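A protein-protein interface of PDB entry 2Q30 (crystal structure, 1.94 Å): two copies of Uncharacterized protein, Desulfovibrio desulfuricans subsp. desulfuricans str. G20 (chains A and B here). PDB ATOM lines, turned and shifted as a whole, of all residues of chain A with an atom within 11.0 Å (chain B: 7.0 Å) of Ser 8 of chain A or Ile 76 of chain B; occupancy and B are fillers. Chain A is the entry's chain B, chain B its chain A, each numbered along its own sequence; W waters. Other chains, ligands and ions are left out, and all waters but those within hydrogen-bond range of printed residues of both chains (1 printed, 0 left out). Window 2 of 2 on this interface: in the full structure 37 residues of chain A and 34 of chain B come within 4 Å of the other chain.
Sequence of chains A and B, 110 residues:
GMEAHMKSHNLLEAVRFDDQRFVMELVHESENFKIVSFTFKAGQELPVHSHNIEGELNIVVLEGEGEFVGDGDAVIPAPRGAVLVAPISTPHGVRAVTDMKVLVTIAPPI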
ATOM      1  N   MET A   6      -1.777 -25.724 -13.472  1.00  0.00           N
ATOM      2  CA  MET A   6      -0.960 -26.975 -13.570  1.00  0.00           C
ATOM      3  C   MET A   6      -1.856 -28.218 -13.438  1.00  0.00           C
ATOM      4  O   MET A   6      -1.839 -29.072 -14.309  1.00  0.00           O
ATOM      5  CB  MET A   6       0.167 -26.973 -12.520  1.00  0.00           C
ATOM      6  CG  MET A   6       1.080 -28.229 -12.426  1.00  0.00           C
ATOM      7  SD  MET A   6       2.139 -28.678 -14.010  1.00  0.00           S
ATOM      8  CE  MET A   6       3.265 -30.094 -13.259  1.00  0.00           C
ATOM      9  N   LYS A   7      -2.627 -28.310 -12.360  1.00  0.00           N
ATOM     10  CA  LYS A   7      -3.505 -29.473 -12.144  1.00  0.00           C
ATOM     11  C   LYS A   7      -4.611 -29.120 -11.154  1.00  0.00           C
ATOM     12  O   LYS A   7      -4.346 -28.510 -10.131  1.00  0.00           O
ATOM     13  CB  LYS A   7      -2.673 -30.663 -11.628  1.00  0.00           C
ATOM     14  CG  LYS A   7      -3.408 -31.983 -11.405  1.00  0.00           C
ATOM     15  CD  LYS A   7      -3.906 -32.604 -12.693  1.00  0.00           C
ATOM     16  CE  LYS A   7      -4.642 -33.912 -12.403  1.00  0.00           C
ATOM     17  NZ  LYS A   7      -5.095 -34.557 -13.665  1.00  0.00           N
ATOM     18  N   SER A   8      -5.847 -29.471 -11.506  1.00  0.00           N
ATOM     19  CA  SER A   8      -6.991 -29.224 -10.651  1.00  0.00           C
ATOM     20  C   SER A   8      -7.683 -30.559 -10.328  1.00  0.00           C
ATOM     21  O   SER A   8      -7.548 -31.556 -11.058  1.00  0.00           O
ATOM     22  CB  SER A   8      -7.946 -28.207 -11.279  1.00  0.00           C
ATOM     23  OG  SER A   8      -8.694 -28.812 -12.285  1.00  0.00           O
ATOM     24  N   HIS A   9      -8.413 -30.554  -9.220  1.00  0.00           N
ATOM     25  CA  HIS A   9      -9.123 -31.728  -8.726  1.00  0.00           C
ATOM     26  C   HIS A   9     -10.498 -31.272  -8.273  1.00  0.00           C
ATOM     27  O   HIS A   9     -10.567 -30.397  -7.433  1.00  0.00           O
ATOM     28  CB  HIS A   9      -8.356 -32.319  -7.525  1.00  0.00           C
ATOM     29  CG  HIS A   9      -6.885 -32.492  -7.761  1.00  0.00           C
ATOM     30  ND1 HIS A   9      -6.327 -33.700  -8.122  1.00  0.00           N
ATOM     31  CD2 HIS A   9      -5.861 -31.602  -7.711  1.00  0.00           C
ATOM     32  CE1 HIS A   9      -5.021 -33.549  -8.273  1.00  0.00           C
ATOM     33  NE2 HIS A   9      -4.713 -32.283  -8.042  1.00  0.00           N
ATOM     34  N   ASN A  10     -11.570 -31.847  -8.812  1.00  0.00           N
ATOM     35  CA  ASN A  10     -12.943 -31.548  -8.397  1.00  0.00           C
ATOM     36  C   ASN A  10     -13.248 -32.521  -7.263  1.00  0.00           C
ATOM     37  O   ASN A  10     -13.765 -33.627  -7.491  1.00  0.00           O
ATOM     38  CB  ASN A  10     -13.922 -31.708  -9.564  1.00  0.00           C
ATOM     39  CG  ASN A  10     -13.667 -30.716 -10.673  1.00  0.00           C
ATOM     40  OD1 ASN A  10     -12.967 -29.724 -10.478  1.00  0.00           O
ATOM     41  ND2 ASN A  10     -14.250 -30.966 -11.842  1.00  0.00           N
ATOM     42  N   LEU A  11     -12.939 -32.083  -6.046  1.00  0.00           N
ATOM     43  CA  LEU A  11     -13.028 -32.934  -4.860  1.00  0.00           C
ATOM     44  C   LEU A  11     -14.438 -33.332  -4.443  1.00  0.00           C
ATOM     45  O   LEU A  11     -14.580 -34.255  -3.651  1.00  0.00           O
ATOM     46  CB  LEU A  11     -12.292 -32.294  -3.684  1.00  0.00           C
ATOM     47  CG  LEU A  11     -10.804 -31.921  -3.889  1.00  0.00           C
ATOM     48  CD1 LEU A  11     -10.318 -31.121  -2.713  1.00  0.00           C
ATOM     49  CD2 LEU A  11      -9.913 -33.132  -4.121  1.00  0.00           C
ATOM     50  N   LEU A  12     -15.465 -32.644  -4.949  1.00  0.00           N
ATOM     51  CA  LEU A  12     -16.869 -33.010  -4.683  1.00  0.00           C
ATOM     52  C   LEU A  12     -17.535 -33.800  -5.842  1.00  0.00           C
ATOM     53  O   LEU A  12     -18.734 -33.958  -5.872  1.00  0.00           O
ATOM     54  CB  LEU A  12     -17.655 -31.760  -4.284  1.00  0.00           C
ATOM     55  CG  LEU A  12     -17.212 -31.149  -2.955  1.00  0.00           C
ATOM     56  CD1 LEU A  12     -18.093 -29.954  -2.638  1.00  0.00           C
ATOM     57  CD2 LEU A  12     -17.250 -32.166  -1.802  1.00  0.00           C
ATOM     58  N   GLU A  13     -16.718 -34.302  -6.759  1.00  0.00           N
ATOM     59  CA  GLU A  13     -17.135 -35.140  -7.863  1.00  0.00           C
ATOM     60  C   GLU A  13     -16.675 -36.563  -7.455  1.00  0.00           C
ATOM     61  O   GLU A  13     -15.596 -36.737  -6.866  1.00  0.00           O
ATOM     62  CB  GLU A  13     -16.415 -34.605  -9.119  1.00  0.00           C
ATOM     63  CG  GLU A  13     -16.831 -35.081 -10.468  1.00  0.00           C
ATOM     64  CD  GLU A  13     -15.917 -34.442 -11.536  1.00  0.00           C
ATOM     65  OE1 GLU A  13     -15.009 -35.153 -12.039  1.00  0.00           O
ATOM     66  OE2 GLU A  13     -16.039 -33.212 -11.785  1.00  0.00           O
ATOM     67  N   LEU A  26      -4.753 -38.900  -1.405  1.00  0.00           N
ATOM     68  CA  LEU A  26      -3.680 -37.945  -1.641  1.00  0.00           C
ATOM     69  C   LEU A  26      -4.110 -37.062  -2.816  1.00  0.00           C
ATOM     70  O   LEU A  26      -4.503 -37.571  -3.884  1.00  0.00           O
ATOM     71  CB  LEU A  26      -2.359 -38.665  -1.995  1.00  0.00           C
ATOM     72  CG  LEU A  26      -1.117 -37.789  -2.219  1.00  0.00           C
ATOM     73  CD1 LEU A  26      -0.720 -37.100  -0.925  1.00  0.00           C
ATOM     74  CD2 LEU A  26       0.035 -38.644  -2.778  1.00  0.00           C
ATOM     75  N   VAL A  27      -4.061 -35.752  -2.624  1.00  0.00           N
ATOM     76  CA  VAL A  27      -4.385 -34.804  -3.707  1.00  0.00           C
ATOM     77  C   VAL A  27      -3.101 -34.357  -4.362  1.00  0.00           C
ATOM     78  O   VAL A  27      -2.983 -34.338  -5.606  1.00  0.00           O
ATOM     79  CB  VAL A  27      -5.260 -33.634  -3.166  1.00  0.00           C
ATOM     80  CG1 VAL A  27      -5.484 -32.545  -4.193  1.00  0.00           C
ATOM     81  CG2 VAL A  27      -6.568 -34.208  -2.703  1.00  0.00           C
ATOM     82  N   HIS A  28      -2.121 -34.009  -3.534  1.00  0.00           N
ATOM     83  CA  HIS A  28      -0.857 -33.492  -4.037  1.00  0.00           C
ATOM     84  C   HIS A  28       0.226 -33.654  -2.991  1.00  0.00           C
ATOM     85  O   HIS A  28      -0.040 -33.545  -1.823  1.00  0.00           O
ATOM     86  CB  HIS A  28      -1.013 -32.000  -4.353  1.00  0.00           C
ATOM     87  CG  HIS A  28       0.217 -31.375  -4.929  1.00  0.00           C
ATOM     88  ND1 HIS A  28       0.582 -31.529  -6.247  1.00  0.00           N
ATOM     89  CD2 HIS A  28       1.148 -30.578  -4.367  1.00  0.00           C
ATOM     90  CE1 HIS A  28       1.702 -30.859  -6.465  1.00  0.00           C
ATOM     91  NE2 HIS A  28       2.057 -30.264  -5.343  1.00  0.00           N
ATOM     92  N   ILE A  35      -1.011 -32.341   0.326  1.00  0.00           N
ATOM     93  CA  ILE A  35      -2.423 -32.025   0.276  1.00  0.00           C
ATOM     94  C   ILE A  35      -3.119 -33.381   0.179  1.00  0.00           C
ATOM     95  O   ILE A  35      -2.852 -34.182  -0.760  1.00  0.00           O
ATOM     96  CB  ILE A  35      -2.822 -31.121  -0.903  1.00  0.00           C
ATOM     97  CG1 ILE A  35      -1.938 -29.843  -0.977  1.00  0.00           C
ATOM     98  CG2 ILE A  35      -4.316 -30.752  -0.762  1.00  0.00           C
ATOM     99  CD1 ILE A  35      -2.124 -29.045  -2.295  1.00  0.00           C
ATOM    100  N   LEU A 103     -10.207 -30.998   3.287  1.00  0.00           N
ATOM    101  CA  LEU A 103      -8.941 -30.917   2.577  1.00  0.00           C
ATOM    102  C   LEU A 103      -7.900 -30.434   3.566  1.00  0.00           C
ATOM    103  O   LEU A 103      -8.091 -29.412   4.224  1.00  0.00           O
ATOM    104  CB  LEU A 103      -9.048 -29.949   1.409  1.00  0.00           C
ATOM    105  CG  LEU A 103      -7.833 -29.894   0.461  1.00  0.00           C
ATOM    106  CD1 LEU A 103      -7.637 -31.190  -0.210  1.00  0.00           C
ATOM    107  CD2 LEU A 103      -8.082 -28.828  -0.579  1.00  0.00           C
ATOM    108  N   GLY B  66     -16.866 -21.128 -10.648  1.00  0.00           N
ATOM    109  CA  GLY B  66     -16.038 -20.268 -11.450  1.00  0.00           C
ATOM    110  C   GLY B  66     -15.122 -21.053 -12.361  1.00  0.00           C
ATOM    111  O   GLY B  66     -15.440 -22.186 -12.778  1.00  0.00           O
ATOM    112  N   GLU B  67     -14.009 -20.413 -12.689  1.00  0.00           N
ATOM    113  CA  GLU B  67     -12.972 -20.970 -13.545  1.00  0.00           C
ATOM    114  C   GLU B  67     -11.606 -20.631 -12.997  1.00  0.00           C
ATOM    115  O   GLU B  67     -11.404 -19.508 -12.497  1.00  0.00           O
ATOM    116  CB  GLU B  67     -13.057 -20.328 -14.931  1.00  0.00           C
ATOM    117  CG  GLU B  67     -14.336 -20.591 -15.605  1.00  0.00           C
ATOM    118  CD  GLU B  67     -14.444 -19.953 -16.957  1.00  0.00           C
ATOM    119  OE1 GLU B  67     -14.165 -18.745 -17.076  1.00  0.00           O
ATOM    120  OE2 GLU B  67     -14.869 -20.648 -17.878  1.00  0.00           O
ATOM    121  N   PHE B  68     -10.681 -21.591 -13.075  1.00  0.00           N
ATOM    122  CA  PHE B  68      -9.273 -21.328 -12.801  1.00  0.00           C
ATOM    123  C   PHE B  68      -8.732 -20.872 -14.128  1.00  0.00           C
ATOM    124  O   PHE B  68      -8.859 -21.586 -15.123  1.00  0.00           O
ATOM    125  CB  PHE B  68      -8.529 -22.573 -12.372  1.00  0.00           C
ATOM    126  CG  PHE B  68      -9.040 -23.155 -11.118  1.00  0.00           C
ATOM    127  CD1 PHE B  68      -9.017 -22.401  -9.939  1.00  0.00           C
ATOM    128  CD2 PHE B  68      -9.510 -24.456 -11.079  1.00  0.00           C
ATOM    129  CE1 PHE B  68      -9.486 -22.934  -8.743  1.00  0.00           C
ATOM    130  CE2 PHE B  68      -9.951 -25.002  -9.882  1.00  0.00           C
ATOM    131  CZ  PHE B  68      -9.954 -24.240  -8.725  1.00  0.00           C
ATOM    132  N   VAL B  69      -8.105 -19.708 -14.154  1.00  0.00           N
ATOM    133  CA  VAL B  69      -7.603 -19.127 -15.402  1.00  0.00           C
ATOM    134  C   VAL B  69      -6.065 -19.235 -15.421  1.00  0.00           C
ATOM    135  O   VAL B  69      -5.411 -19.193 -14.368  1.00  0.00           O
ATOM    136  CB  VAL B  69      -8.091 -17.670 -15.553  1.00  0.00           C
ATOM    137  CG1 VAL B  69      -7.760 -17.099 -16.938  1.00  0.00           C
ATOM    138  CG2 VAL B  69      -9.586 -17.615 -15.326  1.00  0.00           C
ATOM    139  N   GLY B  70      -5.501 -19.409 -16.616  1.00  0.00           N
ATOM    140  CA  GLY B  70      -4.054 -19.518 -16.776  1.00  0.00           C
ATOM    141  C   GLY B  70      -3.542 -18.749 -17.962  1.00  0.00           C
ATOM    142  O   GLY B  70      -4.187 -17.805 -18.444  1.00  0.00           O
ATOM    143  N   ASP B  73      -5.350 -16.914 -21.127  1.00  0.00           N
ATOM    144  CA  ASP B  73      -6.733 -16.903 -20.676  1.00  0.00           C
ATOM    145  C   ASP B  73      -7.395 -18.295 -20.774  1.00  0.00           C
ATOM    146  O   ASP B  73      -8.613 -18.391 -20.851  1.00  0.00           O
ATOM    147  CB  ASP B  73      -7.538 -15.844 -21.455  1.00  0.00           C
ATOM    148  CG  ASP B  73      -8.574 -15.171 -20.602  1.00  0.00           C
ATOM    149  OD1 ASP B  73      -8.148 -14.557 -19.598  1.00  0.00           O
ATOM    150  OD2 ASP B  73      -9.784 -15.201 -20.934  1.00  0.00           O
ATOM    151  N   ALA B  74      -6.587 -19.358 -20.728  1.00  0.00           N
ATOM    152  CA  ALA B  74      -7.077 -20.739 -20.819  1.00  0.00           C
ATOM    153  C   ALA B  74      -7.745 -21.058 -19.485  1.00  0.00           C
ATOM    154  O   ALA B  74      -7.225 -20.654 -18.429  1.00  0.00           O
ATOM    155  CB  ALA B  74      -5.945 -21.689 -21.118  1.00  0.00           C
ATOM    156  N   VAL B  75      -8.880 -21.776 -19.514  1.00  0.00           N
ATOM    157  CA  VAL B  75      -9.653 -22.010 -18.273  1.00  0.00           C
ATOM    158  C   VAL B  75      -9.924 -23.466 -17.922  1.00  0.00           C
ATOM    159  O   VAL B  75     -10.053 -24.305 -18.808  1.00  0.00           O
ATOM    160  CB  VAL B  75     -11.017 -21.252 -18.293  1.00  0.00           C
ATOM    161  CG1 VAL B  75     -10.785 -19.744 -18.430  1.00  0.00           C
ATOM    162  CG2 VAL B  75     -11.923 -21.769 -19.408  1.00  0.00           C
ATOM    163  N   ILE B  76      -9.994 -23.722 -16.614  1.00  0.00           N
ATOM    164  CA  ILE B  76     -10.331 -25.014 -16.043  1.00  0.00           C
ATOM    165  C   ILE B  76     -11.584 -24.740 -15.202  1.00  0.00           C
ATOM    166  O   ILE B  76     -11.545 -23.840 -14.350  1.00  0.00           O
ATOM    167  CB  ILE B  76      -9.239 -25.561 -15.121  1.00  0.00           C
ATOM    168  CG1 ILE B  76      -7.929 -25.778 -15.901  1.00  0.00           C
ATOM    169  CG2 ILE B  76      -9.711 -26.861 -14.467  1.00  0.00           C
ATOM    170  CD1 ILE B  76      -6.740 -26.276 -15.026  1.00  0.00           C
ATOM    171  N   PRO B  77     -12.687 -25.481 -15.431  1.00  0.00           N
ATOM    172  CA  PRO B  77     -13.868 -25.247 -14.603  1.00  0.00           C
ATOM    173  C   PRO B  77     -13.543 -25.433 -13.131  1.00  0.00           C
ATOM    174  O   PRO B  77     -12.783 -26.323 -12.779  1.00  0.00           O
ATOM    175  CB  PRO B  77     -14.863 -26.299 -15.097  1.00  0.00           C
ATOM    176  CG  PRO B  77     -14.469 -26.542 -16.506  1.00  0.00           C
ATOM    177  CD  PRO B  77     -12.968 -26.490 -16.480  1.00  0.00           C
ATOM    178  N   ALA B  78     -14.078 -24.555 -12.303  1.00  0.00           N
ATOM    179  CA  ALA B  78     -13.785 -24.520 -10.888  1.00  0.00           C
ATOM    180  C   ALA B  78     -15.110 -24.589 -10.128  1.00  0.00           C
ATOM    181  O   ALA B  78     -15.587 -23.587  -9.594  1.00  0.00           O
ATOM    182  CB  ALA B  78     -13.002 -23.249 -10.566  1.00  0.00           C
ATOM    183  N   PRO B  79     -15.746 -25.775 -10.119  1.00  0.00           N
ATOM    184  CA  PRO B  79     -16.964 -25.903  -9.360  1.00  0.00           C
ATOM    185  C   PRO B  79     -16.652 -25.858  -7.866  1.00  0.00           C
ATOM    186  O   PRO B  79     -15.489 -25.948  -7.476  1.00  0.00           O
ATOM    187  CB  PRO B  79     -17.486 -27.281  -9.779  1.00  0.00           C
ATOM    188  CG  PRO B  79     -16.251 -28.048 -10.075  1.00  0.00           C
ATOM    189  CD  PRO B  79     -15.402 -27.044 -10.791  1.00  0.00           C
ATOM    190  N   ALA B  82     -13.627 -27.595  -5.919  1.00  0.00           N
ATOM    191  CA  ALA B  82     -12.502 -27.833  -6.813  1.00  0.00           C
ATOM    192  C   ALA B  82     -11.276 -27.219  -6.193  1.00  0.00           C
ATOM    193  O   ALA B  82     -11.373 -26.213  -5.478  1.00  0.00           O
ATOM    194  CB  ALA B  82     -12.752 -27.257  -8.214  1.00  0.00           C
ATOM    195  N   VAL B  83     -10.118 -27.853  -6.424  1.00  0.00           N
ATOM    196  CA  VAL B  83      -8.837 -27.352  -5.938  1.00  0.00           C
ATOM    197  C   VAL B  83      -7.857 -27.321  -7.088  1.00  0.00           C
ATOM    198  O   VAL B  83      -7.751 -28.298  -7.806  1.00  0.00           O
ATOM    199  CB  VAL B  83      -8.246 -28.190  -4.735  1.00  0.00           C
ATOM    200  CG1 VAL B  83      -8.098 -29.621  -5.062  1.00  0.00           C
ATOM    201  CG2 VAL B  83      -6.907 -27.623  -4.280  1.00  0.00           C
ATOM    202  N   LEU B  84      -7.193 -26.182  -7.271  1.00  0.00           N
ATOM    203  CA  LEU B  84      -6.148 -26.003  -8.269  1.00  0.00           C
ATOM    204  C   LEU B  84      -4.858 -26.049  -7.488  1.00  0.00           C
ATOM    205  O   LEU B  84      -4.812 -25.428  -6.448  1.00  0.00           O
ATOM    206  CB  LEU B  84      -6.258 -24.626  -8.894  1.00  0.00           C
ATOM    207  CG  LEU B  84      -5.175 -24.196  -9.894  1.00  0.00           C
ATOM    208  CD1 LEU B  84      -5.291 -24.962 -11.173  1.00  0.00           C
ATOM    209  CD2 LEU B  84      -5.335 -22.696 -10.117  1.00  0.00           C
ATOM    210  N   VAL B  85      -3.847 -26.786  -7.969  1.00  0.00           N
ATOM    211  CA  VAL B  85      -2.507 -26.767  -7.389  1.00  0.00           C
ATOM    212  C   VAL B  85      -1.554 -26.322  -8.497  1.00  0.00           C
ATOM    213  O   VAL B  85      -1.579 -26.865  -9.596  1.00  0.00           O
ATOM    214  CB  VAL B  85      -2.034 -28.113  -6.814  1.00  0.00           C
ATOM    215  CG1 VAL B  85      -0.690 -27.908  -5.987  1.00  0.00           C
ATOM    216  CG2 VAL B  85      -3.089 -28.708  -5.909  1.00  0.00           C
HETATM  217  O   HOH W   1     -11.328 -28.150 -11.624  1.00  0.00           O
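The backbone NH (N) of His 9 of chain A sits at hydrogen-bond distance from the backbone carbonyl oxygen (O) of Val 83 of chain B (2.7 Å).
The backbone carbonyl oxygen of Lys 7 of chain A is in hydrogen-bond range of the backbone NH of Val 85 of chain B (2.8 Å).
O of Val 85 of chain B touches CB of Met 6 of chain A, at 3.4 Å.
Leu 84 of chain B touches Lys 7 of chain A (CA to O, 3.6 Å).
OG of Ser 8 of chain A touches CG2 of Ile 76 of chain B, at 3.1 Å.
Ser 8 of chain A touches Val 83 of chain B.
His 9 of chain A touches Ala 82 of chain B (O to CA, 3.3 Å).
Pro 79 of chain B touches Asn 10 of chain A (CD to OD1, 3.6 Å).
CB of Ala 82 of chain B touches OD1 of Asn 10 of chain A, at 3.4 Å.
Val 83 of chain B touches Leu 11 of chain A.
His 28 of chain A touches Val 85 of chain B.
CG2 of Val 85 of chain B touches CD1 of Ile 35 of chain A, at 3.8 Å.
N of Phe 68 of chain B sits at hydrogen-bond distance from O of Ile 76 of chain B, 2.7 Å away.
The side-chain amide nitrogen (ND2) of Asn 10 of chain A lies within hydrogen-bond range of the side-chain carboxylate (OE2) of Glu 13 of chain A (2.9 Å).
The backbone NH (N) of Val 27 of chain A is in hydrogen-bond range of the backbone carbonyl oxygen (O) of Ile 35 of chain A.
N of Ile 35 of chain A sits at hydrogen-bond distance from O of His 28 of chain A (2.6 Å).
Printed residues of chain A that touch a printed residue of chain B: Met 6, Lys 7, Ser 8, His 9, Asn 10, Leu 11, His 28 and Ile 35.
Hydrophobic or aromatic side chains of chain A within 4 Å of the printed part of chain B: Met 6, His 9, Leu 11, His 28 and Ile 35.
Of the 16 printed residues of chain B, 6 touch a printed residue of chain A.
Among the printed residues, 12 pairs touch across the chains.
No position is printed for both chains.
Of the printed residues of chain B, Met 6 of chain A touches Val 85.
Printed residues of chain B within 4 Å of Lys 7 of chain A: Leu 84 and Val 85.
Ser 8 of chain A touches two residues of chain B.
Of the printed residues of chain B, His 9 of chain A touches Ala 82 and Val 83.
Glu 13 of chain A touches none of the printed residues of chain B.
Val 27 of chain A touches none of the printed residues of chain B.
No residue of chain A comes within 4 Å of Glu 67 of chain B.
No residue of chain A comes within 4 Å of Phe 68 of chain B.
Ala 74 of chain B touches none of the printed residues of chain A.
Val 75 of chain B touches none of the printed residues of chain A.
Ile 76 of chain B touches one residue of chain A.
No residue of chain A comes within 4 Å of Pro 77 of chain B.
No residue of chain A comes within 4 Å of Ala 78 of chain B.
Printed residues of chain A within 4 Å of Val 83 of chain B: Ser 8, His 9 and Leu 11.
Of the printed residues of chain A, Val 85 of chain B touches Met 6, Lys 7, His 28 and Ile 35.
Water W1 lies within hydrogen-bond range of the side-chain amide oxygen (OD1) of Asn 10 of chain A (2.5 Å), the backbone carbonyl oxygen (O) of Pro 77 of chain B (2.6 Å) and the side-chain hydroxyl (OG) of Ser 8 of chain A (2.8 Å).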
